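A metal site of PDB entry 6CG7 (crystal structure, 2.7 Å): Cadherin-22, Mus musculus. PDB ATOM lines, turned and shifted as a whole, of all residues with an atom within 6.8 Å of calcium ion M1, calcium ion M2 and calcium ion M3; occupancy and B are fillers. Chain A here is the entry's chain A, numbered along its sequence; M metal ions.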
ATOM      1  N   GLU A  11      -7.243  -8.051 -34.797  1.00  0.00           N
ATOM      2  CA  GLU A  11      -6.921  -6.646 -34.884  1.00  0.00           C
ATOM      3  C   GLU A  11      -5.690  -6.426 -35.775  1.00  0.00           C
ATOM      4  O   GLU A  11      -4.985  -7.366 -36.151  1.00  0.00           O
ATOM      5  CB  GLU A  11      -6.650  -6.042 -33.499  1.00  0.00           C
ATOM      6  CG  GLU A  11      -5.404  -6.584 -32.807  1.00  0.00           C
ATOM      7  CD  GLU A  11      -4.978  -5.716 -31.628  1.00  0.00           C
ATOM      8  OE1 GLU A  11      -4.499  -6.273 -30.614  1.00  0.00           O
ATOM      9  OE2 GLU A  11      -5.111  -4.477 -31.724  1.00  0.00           O
ATOM     10  N   GLU A  12      -5.459  -5.160 -36.099  1.00  0.00           N
ATOM     11  CA  GLU A  12      -4.284  -4.726 -36.842  1.00  0.00           C
ATOM     12  C   GLU A  12      -4.063  -5.569 -38.099  1.00  0.00           C
ATOM     13  O   GLU A  12      -2.955  -5.999 -38.400  1.00  0.00           O
ATOM     14  CB  GLU A  12      -3.035  -4.752 -35.953  1.00  0.00           C
ATOM     15  CG  GLU A  12      -3.221  -4.186 -34.559  1.00  0.00           C
ATOM     16  CD  GLU A  12      -3.514  -2.695 -34.563  1.00  0.00           C
ATOM     17  OE1 GLU A  12      -3.230  -2.040 -35.585  1.00  0.00           O
ATOM     18  OE2 GLU A  12      -4.041  -2.180 -33.549  1.00  0.00           O
ATOM     19  N   LEU A  63      -8.571  -2.753 -37.574  1.00  0.00           N
ATOM     20  CA  LEU A  63      -9.178  -2.628 -36.254  1.00  0.00           C
ATOM     21  C   LEU A  63      -8.089  -2.612 -35.177  1.00  0.00           C
ATOM     22  O   LEU A  63      -7.023  -3.209 -35.341  1.00  0.00           O
ATOM     23  CB  LEU A  63     -10.151  -3.770 -35.994  1.00  0.00           C
ATOM     24  CG  LEU A  63     -11.359  -3.868 -36.933  1.00  0.00           C
ATOM     25  CD1 LEU A  63     -12.142  -5.146 -36.652  1.00  0.00           C
ATOM     26  CD2 LEU A  63     -12.260  -2.658 -36.812  1.00  0.00           C
ATOM     27  N   ASP A  64      -8.385  -1.928 -34.076  1.00  0.00           N
ATOM     28  CA  ASP A  64      -7.452  -1.769 -32.964  1.00  0.00           C
ATOM     29  C   ASP A  64      -8.163  -2.130 -31.667  1.00  0.00           C
ATOM     30  O   ASP A  64      -9.067  -1.418 -31.240  1.00  0.00           O
ATOM     31  CB  ASP A  64      -6.906  -0.346 -32.915  1.00  0.00           C
ATOM     32  CG  ASP A  64      -5.889  -0.135 -31.808  1.00  0.00           C
ATOM     33  OD1 ASP A  64      -5.320  -1.138 -31.324  1.00  0.00           O
ATOM     34  OD2 ASP A  64      -5.651   1.027 -31.430  1.00  0.00           O
ATOM     35  N   ARG A  65      -7.744  -3.241 -31.041  1.00  0.00           N
ATOM     36  CA  ARG A  65      -8.383  -3.669 -29.807  1.00  0.00           C
ATOM     37  C   ARG A  65      -8.099  -2.704 -28.669  1.00  0.00           C
ATOM     38  O   ARG A  65      -8.954  -2.470 -27.806  1.00  0.00           O
ATOM     39  CB  ARG A  65      -7.909  -5.070 -29.431  1.00  0.00           C
ATOM     40  CG  ARG A  65      -8.768  -5.762 -28.390  1.00  0.00           C
ATOM     41  CD  ARG A  65      -8.034  -6.917 -27.727  1.00  0.00           C
ATOM     42  NE  ARG A  65      -6.917  -6.434 -26.921  1.00  0.00           N
ATOM     43  CZ  ARG A  65      -7.045  -5.925 -25.702  1.00  0.00           C
ATOM     44  NH1 ARG A  65      -8.250  -5.831 -25.134  1.00  0.00           N
ATOM     45  NH2 ARG A  65      -5.975  -5.508 -25.036  1.00  0.00           N
ATOM     46  N   GLU A  66      -6.896  -2.119 -28.653  1.00  0.00           N
ATOM     47  CA  GLU A  66      -6.557  -1.126 -27.645  1.00  0.00           C
ATOM     48  C   GLU A  66      -7.343   0.161 -27.807  1.00  0.00           C
ATOM     49  O   GLU A  66      -7.320   1.002 -26.911  1.00  0.00           O
ATOM     50  CB  GLU A  66      -5.051  -0.838 -27.663  1.00  0.00           C
ATOM     51  CG  GLU A  66      -4.186  -1.954 -27.089  1.00  0.00           C
ATOM     52  CD  GLU A  66      -4.190  -3.213 -27.940  1.00  0.00           C
ATOM     53  OE1 GLU A  66      -4.149  -3.094 -29.186  1.00  0.00           O
ATOM     54  OE2 GLU A  66      -4.232  -4.318 -27.368  1.00  0.00           O
ATOM     55  N   GLN A  67      -8.017   0.348 -28.944  1.00  0.00           N
ATOM     56  CA  GLN A  67      -8.943   1.457 -29.137  1.00  0.00           C
ATOM     57  C   GLN A  67     -10.367   1.053 -28.802  1.00  0.00           C
ATOM     58  O   GLN A  67     -11.060   1.760 -28.068  1.00  0.00           O
ATOM     59  CB  GLN A  67      -8.860   1.963 -30.584  1.00  0.00           C
ATOM     60  CG  GLN A  67      -9.742   3.173 -30.885  1.00  0.00           C
ATOM     61  CD  GLN A  67     -10.312   3.153 -32.295  1.00  0.00           C
ATOM     62  OE1 GLN A  67     -10.181   2.166 -33.023  1.00  0.00           O
ATOM     63  NE2 GLN A  67     -10.959   4.249 -32.681  1.00  0.00           N
ATOM     64  N   GLN A  97     -10.093  -9.599 -31.749  1.00  0.00           N
ATOM     65  CA  GLN A  97      -9.166 -10.368 -30.945  1.00  0.00           C
ATOM     66  C   GLN A  97      -7.816  -9.666 -30.838  1.00  0.00           C
ATOM     67  O   GLN A  97      -7.444  -8.831 -31.673  1.00  0.00           O
ATOM     68  CB  GLN A  97      -8.990 -11.777 -31.522  1.00  0.00           C
ATOM     69  CG  GLN A  97      -8.178 -12.737 -30.638  1.00  0.00           C
ATOM     70  CD  GLN A  97      -8.760 -12.890 -29.238  1.00  0.00           C
ATOM     71  OE1 GLN A  97      -8.134 -12.522 -28.248  1.00  0.00           O
ATOM     72  NE2 GLN A  97      -9.959 -13.445 -29.162  1.00  0.00           N
ATOM     73  N   ASP A  98      -7.068 -10.015 -29.791  1.00  0.00           N
ATOM     74  CA  ASP A  98      -5.840  -9.343 -29.428  1.00  0.00           C
ATOM     75  C   ASP A  98      -4.635  -9.937 -30.153  1.00  0.00           C
ATOM     76  O   ASP A  98      -4.590 -11.142 -30.418  1.00  0.00           O
ATOM     77  CB  ASP A  98      -5.614  -9.446 -27.912  1.00  0.00           C
ATOM     78  CG  ASP A  98      -4.319  -8.831 -27.463  1.00  0.00           C
ATOM     79  OD1 ASP A  98      -4.193  -7.590 -27.567  1.00  0.00           O
ATOM     80  OD2 ASP A  98      -3.428  -9.574 -27.013  1.00  0.00           O
ATOM     81  N   ILE A  99      -3.681  -9.069 -30.480  1.00  0.00           N
ATOM     82  CA  ILE A  99      -2.353  -9.491 -30.913  1.00  0.00           C
ATOM     83  C   ILE A  99      -1.339  -8.733 -30.066  1.00  0.00           C
ATOM     84  O   ILE A  99      -1.608  -7.659 -29.526  1.00  0.00           O
ATOM     85  CB  ILE A  99      -2.091  -9.228 -32.416  1.00  0.00           C
ATOM     86  CG1 ILE A  99      -1.972  -7.729 -32.707  1.00  0.00           C
ATOM     87  CG2 ILE A  99      -3.191  -9.873 -33.263  1.00  0.00           C
ATOM     88  CD1 ILE A  99      -1.569  -7.392 -34.113  1.00  0.00           C
ATOM     89  N   ASN A 100      -0.146  -9.315 -29.942  1.00  0.00           N
ATOM     90  CA  ASN A 100       0.927  -8.722 -29.139  1.00  0.00           C
ATOM     91  C   ASN A 100       1.554  -7.580 -29.934  1.00  0.00           C
ATOM     92  O   ASN A 100       2.596  -7.724 -30.592  1.00  0.00           O
ATOM     93  CB  ASN A 100       1.952  -9.765 -28.753  1.00  0.00           C
ATOM     94  CG  ASN A 100       3.016  -9.218 -27.828  1.00  0.00           C
ATOM     95  OD1 ASN A 100       2.792  -8.236 -27.122  1.00  0.00           O
ATOM     96  ND2 ASN A 100       4.194  -9.842 -27.834  1.00  0.00           N
ATOM     97  N   ASP A 101       0.913  -6.408 -29.857  1.00  0.00           N
ATOM     98  CA  ASP A 101       1.405  -5.214 -30.542  1.00  0.00           C
ATOM     99  C   ASP A 101       1.548  -4.030 -29.588  1.00  0.00           C
ATOM    100  O   ASP A 101       1.563  -2.878 -30.040  1.00  0.00           O
ATOM    101  CB  ASP A 101       0.492  -4.847 -31.710  1.00  0.00           C
ATOM    102  CG  ASP A 101      -0.892  -4.414 -31.247  1.00  0.00           C
ATOM    103  OD1 ASP A 101      -1.453  -3.480 -31.854  1.00  0.00           O
ATOM    104  OD2 ASP A 101      -1.415  -5.014 -30.289  1.00  0.00           O
ATOM    105  N   SER A 102       1.662  -4.276 -28.287  1.00  0.00           N
ATOM    106  CA  SER A 102       1.858  -3.228 -27.291  1.00  0.00           C
ATOM    107  C   SER A 102       3.102  -3.542 -26.481  1.00  0.00           C
ATOM    108  O   SER A 102       3.179  -4.591 -25.843  1.00  0.00           O
ATOM    109  CB  SER A 102       0.629  -3.112 -26.377  1.00  0.00           C
ATOM    110  OG  SER A 102      -0.554  -2.920 -27.122  1.00  0.00           O
ATOM    111  N   GLU A 103       4.078  -2.632 -26.505  1.00  0.00           N
ATOM    112  CA  GLU A 103       5.298  -2.820 -25.740  1.00  0.00           C
ATOM    113  C   GLU A 103       5.024  -2.637 -24.241  1.00  0.00           C
ATOM    114  O   GLU A 103       4.152  -1.853 -23.860  1.00  0.00           O
ATOM    115  CB  GLU A 103       6.376  -1.839 -26.177  1.00  0.00           C
ATOM    116  CG  GLU A 103       6.970  -2.090 -27.550  1.00  0.00           C
ATOM    117  CD  GLU A 103       8.302  -1.392 -27.747  1.00  0.00           C
ATOM    118  OE1 GLU A 103       8.806  -0.768 -26.782  1.00  0.00           O
ATOM    119  OE2 GLU A 103       8.853  -1.466 -28.864  1.00  0.00           O
ATOM    120  N   PRO A 104       5.754  -3.350 -23.381  1.00  0.00           N
ATOM    121  CA  PRO A 104       5.679  -3.044 -21.953  1.00  0.00           C
ATOM    122  C   PRO A 104       6.235  -1.664 -21.667  1.00  0.00           C
ATOM    123  O   PRO A 104       7.214  -1.232 -22.278  1.00  0.00           O
ATOM    124  CB  PRO A 104       6.530  -4.145 -21.296  1.00  0.00           C
ATOM    125  CG  PRO A 104       6.625  -5.214 -22.320  1.00  0.00           C
ATOM    126  CD  PRO A 104       6.604  -4.524 -23.642  1.00  0.00           C
ATOM    127  N   ASP A 132       1.300  -3.625 -19.677  1.00  0.00           N
ATOM    128  CA  ASP A 132       1.181  -4.058 -21.070  1.00  0.00           C
ATOM    129  C   ASP A 132      -0.265  -3.896 -21.489  1.00  0.00           C
ATOM    130  O   ASP A 132      -1.167  -4.491 -20.881  1.00  0.00           O
ATOM    131  CB  ASP A 132       1.635  -5.511 -21.231  1.00  0.00           C
ATOM    132  CG  ASP A 132       1.923  -5.881 -22.667  1.00  0.00           C
ATOM    133  OD1 ASP A 132       3.047  -6.337 -22.946  1.00  0.00           O
ATOM    134  OD2 ASP A 132       1.025  -5.718 -23.522  1.00  0.00           O
ATOM    135  N   ALA A 133      -0.499  -3.088 -22.523  1.00  0.00           N
ATOM    136  CA  ALA A 133      -1.862  -2.768 -22.939  1.00  0.00           C
ATOM    137  C   ALA A 133      -2.551  -3.921 -23.653  1.00  0.00           C
ATOM    138  O   ALA A 133      -3.734  -3.789 -23.984  1.00  0.00           O
ATOM    139  CB  ALA A 133      -1.849  -1.539 -23.853  1.00  0.00           C
ATOM    140  N   ASP A 134      -1.860  -5.031 -23.903  1.00  0.00           N
ATOM    141  CA  ASP A 134      -2.459  -6.155 -24.598  1.00  0.00           C
ATOM    142  C   ASP A 134      -3.402  -6.912 -23.657  1.00  0.00           C
ATOM    143  O   ASP A 134      -3.587  -6.555 -22.492  1.00  0.00           O
ATOM    144  CB  ASP A 134      -1.373  -7.067 -25.160  1.00  0.00           C
ATOM    145  CG  ASP A 134      -0.569  -6.403 -26.274  1.00  0.00           C
ATOM    146  OD1 ASP A 134      -1.158  -5.595 -27.026  1.00  0.00           O
ATOM    147  OD2 ASP A 134       0.635  -6.686 -26.395  1.00  0.00           O
ATOM    148  N   ASP A 135      -3.997  -7.990 -24.169  1.00  0.00           N
ATOM    149  CA  ASP A 135      -4.980  -8.768 -23.424  1.00  0.00           C
ATOM    150  C   ASP A 135      -4.299  -9.712 -22.447  1.00  0.00           C
ATOM    151  O   ASP A 135      -3.604 -10.654 -22.880  1.00  0.00           O
ATOM    152  CB  ASP A 135      -5.874  -9.564 -24.383  1.00  0.00           C
ATOM    153  CG  ASP A 135      -7.109 -10.127 -23.698  1.00  0.00           C
ATOM    154  OD1 ASP A 135      -8.129 -10.353 -24.381  1.00  0.00           O
ATOM    155  OD2 ASP A 135      -7.072 -10.323 -22.459  1.00  0.00           O
ATOM    156  N   SER A 140       0.116 -15.056 -23.829  1.00  0.00           N
ATOM    157  CA  SER A 140       1.147 -14.396 -23.039  1.00  0.00           C
ATOM    158  C   SER A 140       1.465 -12.997 -23.546  1.00  0.00           C
ATOM    159  O   SER A 140       2.540 -12.467 -23.256  1.00  0.00           O
ATOM    160  CB  SER A 140       2.422 -15.257 -23.020  1.00  0.00           C
ATOM    161  OG  SER A 140       2.173 -16.532 -22.457  1.00  0.00           O
ATOM    162  N   SER A 141       0.538 -12.391 -24.296  1.00  0.00           N
ATOM    163  CA  SER A 141       0.784 -11.068 -24.863  1.00  0.00           C
ATOM    164  C   SER A 141       1.017 -10.011 -23.790  1.00  0.00           C
ATOM    165  O   SER A 141       1.610  -8.970 -24.081  1.00  0.00           O
ATOM    166  CB  SER A 141      -0.401 -10.651 -25.752  1.00  0.00           C
ATOM    167  OG  SER A 141      -0.610 -11.576 -26.794  1.00  0.00           O
ATOM    168  N   ALA A 142       0.557 -10.256 -22.556  1.00  0.00           N
ATOM    169  CA  ALA A 142       0.726  -9.313 -21.471  1.00  0.00           C
ATOM    170  C   ALA A 142       1.390  -9.928 -20.245  1.00  0.00           C
ATOM    171  O   ALA A 142       1.375  -9.316 -19.175  1.00  0.00           O
ATOM    172  CB  ALA A 142      -0.621  -8.699 -21.077  1.00  0.00           C
ATOM    173  N   ARG A 143       1.946 -11.135 -20.366  1.00  0.00           N
ATOM    174  CA  ARG A 143       2.666 -11.774 -19.273  1.00  0.00           C
ATOM    175  C   ARG A 143       4.135 -11.403 -19.380  1.00  0.00           C
ATOM    176  O   ARG A 143       4.814 -11.805 -20.327  1.00  0.00           O
ATOM    177  CB  ARG A 143       2.455 -13.292 -19.297  1.00  0.00           C
ATOM    178  CG  ARG A 143       1.033 -13.689 -18.968  1.00  0.00           C
ATOM    179  CD  ARG A 143       0.819 -15.191 -18.988  1.00  0.00           C
ATOM    180  NE  ARG A 143      -0.607 -15.515 -18.854  1.00  0.00           N
ATOM    181  CZ  ARG A 143      -1.114 -16.740 -18.932  1.00  0.00           C
ATOM    182  NH1 ARG A 143      -0.315 -17.785 -19.142  1.00  0.00           N
ATOM    183  NH2 ARG A 143      -2.421 -16.928 -18.795  1.00  0.00           N
ATOM    184  N   LEU A 144       4.632 -10.628 -18.420  1.00  0.00           N
ATOM    185  CA  LEU A 144       5.919  -9.974 -18.521  1.00  0.00           C
ATOM    186  C   LEU A 144       6.992 -10.725 -17.726  1.00  0.00           C
ATOM    187  O   LEU A 144       6.708 -11.479 -16.803  1.00  0.00           O
ATOM    188  CB  LEU A 144       5.820  -8.532 -18.008  1.00  0.00           C
ATOM    189  CG  LEU A 144       4.720  -7.684 -18.666  1.00  0.00           C
ATOM    190  CD1 LEU A 144       4.670  -6.306 -18.033  1.00  0.00           C
ATOM    191  CD2 LEU A 144       4.920  -7.581 -20.167  1.00  0.00           C
ATOM    192  N   ASP A 187       7.448  -9.116 -22.674  1.00  0.00           N
ATOM    193  CA  ASP A 187       6.225  -9.916 -22.694  1.00  0.00           C
ATOM    194  C   ASP A 187       6.487 -11.258 -23.374  1.00  0.00           C
ATOM    195  O   ASP A 187       7.643 -11.663 -23.573  1.00  0.00           O
ATOM    196  CB  ASP A 187       5.094  -9.116 -23.359  1.00  0.00           C
ATOM    197  CG  ASP A 187       5.424  -8.708 -24.782  1.00  0.00           C
ATOM    198  OD1 ASP A 187       6.234  -9.399 -25.435  1.00  0.00           O
ATOM    199  OD2 ASP A 187       4.853  -7.692 -25.248  1.00  0.00           O
ATOM    200  N   MET A 188       5.419 -11.964 -23.744  1.00  0.00           N
ATOM    201  CA  MET A 188       5.514 -13.325 -24.269  1.00  0.00           C
ATOM    202  C   MET A 188       6.256 -14.264 -23.331  1.00  0.00           C
ATOM    203  O   MET A 188       6.801 -15.283 -23.768  1.00  0.00           O
ATOM    204  CB  MET A 188       6.175 -13.337 -25.657  1.00  0.00           C
ATOM    205  CG  MET A 188       5.410 -12.597 -26.734  1.00  0.00           C
ATOM    206  SD  MET A 188       3.774 -13.266 -27.084  1.00  0.00           S
ATOM    207  CE  MET A 188       4.184 -14.933 -27.617  1.00  0.00           C
ATOM    208  N   LEU A 195       8.041  -8.323 -27.094  1.00  0.00           N
ATOM    209  CA  LEU A 195       8.327  -6.903 -27.038  1.00  0.00           C
ATOM    210  C   LEU A 195       8.918  -6.528 -25.674  1.00  0.00           C
ATOM    211  O   LEU A 195       8.746  -7.247 -24.682  1.00  0.00           O
ATOM    212  CB  LEU A 195       7.054  -6.102 -27.307  1.00  0.00           C
ATOM    213  CG  LEU A 195       6.284  -6.506 -28.567  1.00  0.00           C
ATOM    214  CD1 LEU A 195       4.982  -5.734 -28.681  1.00  0.00           C
ATOM    215  CD2 LEU A 195       7.138  -6.305 -29.807  1.00  0.00           C
HETATM  216 CA    CA M   1      -2.921  -5.842 -28.635  1.00  0.00          CA
HETATM  217 CA    CA M   2      -3.490  -2.491 -31.255  1.00  0.00          CA
HETATM  218 CA    CA M   3       2.596  -6.926 -25.145  1.00  0.00          CA
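The side-chain carboxylate (OE2) of Glu 66 binds calcium ion M1, at 2.4 Å.
OD2 of Asp 101 is bound to calcium ion M1 (2.4 Å).
Calcium ion M1 is bound by OD1 of Asp 134, at 2.4 Å.
Calcium ion M1 is bound by OD1 of Asp 98 (2.4 Å).
O of Ile 99 binds calcium ion M1 (2.4 Å).
The side-chain carboxylate (OE1) of Glu 11 is bound to calcium ion M1, at 2.6 Å.
Slightly farther from calcium ion M1 lies the side-chain carboxylate (OE1) of Glu 66 (3.1 Å).
The side-chain carboxylate (OD1) of Asp 98 sits close to the guanidinium group (NE) of Arg 65, at 3.0 Å.
N of Arg 65 sits close to OE2 of Glu 11.
The side-chain carboxylate of Asp 98 sits at hydrogen-bond distance from the backbone NH of Asp 135.
The backbone carbonyl oxygen (O) of Gln 97 lies within hydrogen-bond range of the backbone NH (N) of Glu 11, at 3.2 Å.
The backbone NH (N) of Glu 12 sits at hydrogen-bond distance from the backbone carbonyl oxygen (O) of Leu 63, 2.6 Å away.
The side-chain carboxylate of Asp 187 is in hydrogen-bond range of the backbone NH of Leu 195.
The side-chain amide nitrogen (ND2) of Asn 100 lies close to the side-chain sulfur (SD) of Met 188.
The side-chain hydroxyl of Ser 141 lies close to the side-chain carboxylate of Asp 98.
Of the 27 residues printed, 5 come within 4 Å of calcium ion M2.
The nearest printed residue that does not touch calcium ion M2 is Arg 65 (4.3 Å).
Six residues have an atom within 4 Å of calcium ion M3: Asn 100, Ser 102, Asp 132, Asp 134, Ser 141 and Asp 187.
Along chain A the residues within 4 Å of calcium ion M3 span positions 100 to 187.
The nearest printed residue that does not touch calcium ion M3 is Leu 195 (4.4 Å).
Calcium ion M2 is bound by the side-chain carboxylate (OE1) of Glu 66.
The side-chain carboxylate (OD1) of Asp 64 is bound to calcium ion M2.
Calcium ion M2 is bound by OD1 of Asp 101, at 2.3 Å.
Calcium ion M2 is bound by OE2 of Glu 12 (2.4 Å).
The side-chain carboxylate (OE2) of Glu 11 binds calcium ion M2, 2.6 Å away.
Calcium ion M2 has five donor atoms within binding distance.
Calcium ion M3 is bound by the side-chain carboxylate (OD1) of Asp 132 (2.3 Å), the side-chain carboxylate (OD2) of Asp 134 (2.3 Å), the side-chain amide oxygen (OD1) of Asn 100 (2.4 Å), the side-chain carboxylate (OD2) of Asp 187 (2.4 Å), the backbone carbonyl oxygen (O) of Ser 102 (2.5 Å), the backbone carbonyl oxygen (O) of Ser 141 (2.5 Å) and the side-chain carboxylate (OD2) of Asp 132 (2.6 Å).
Six residues have an atom within 4 Å of calcium ion M1: Glu 11, Glu 66, Asp 98, Ile 99, Asp 101 and Asp 134.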
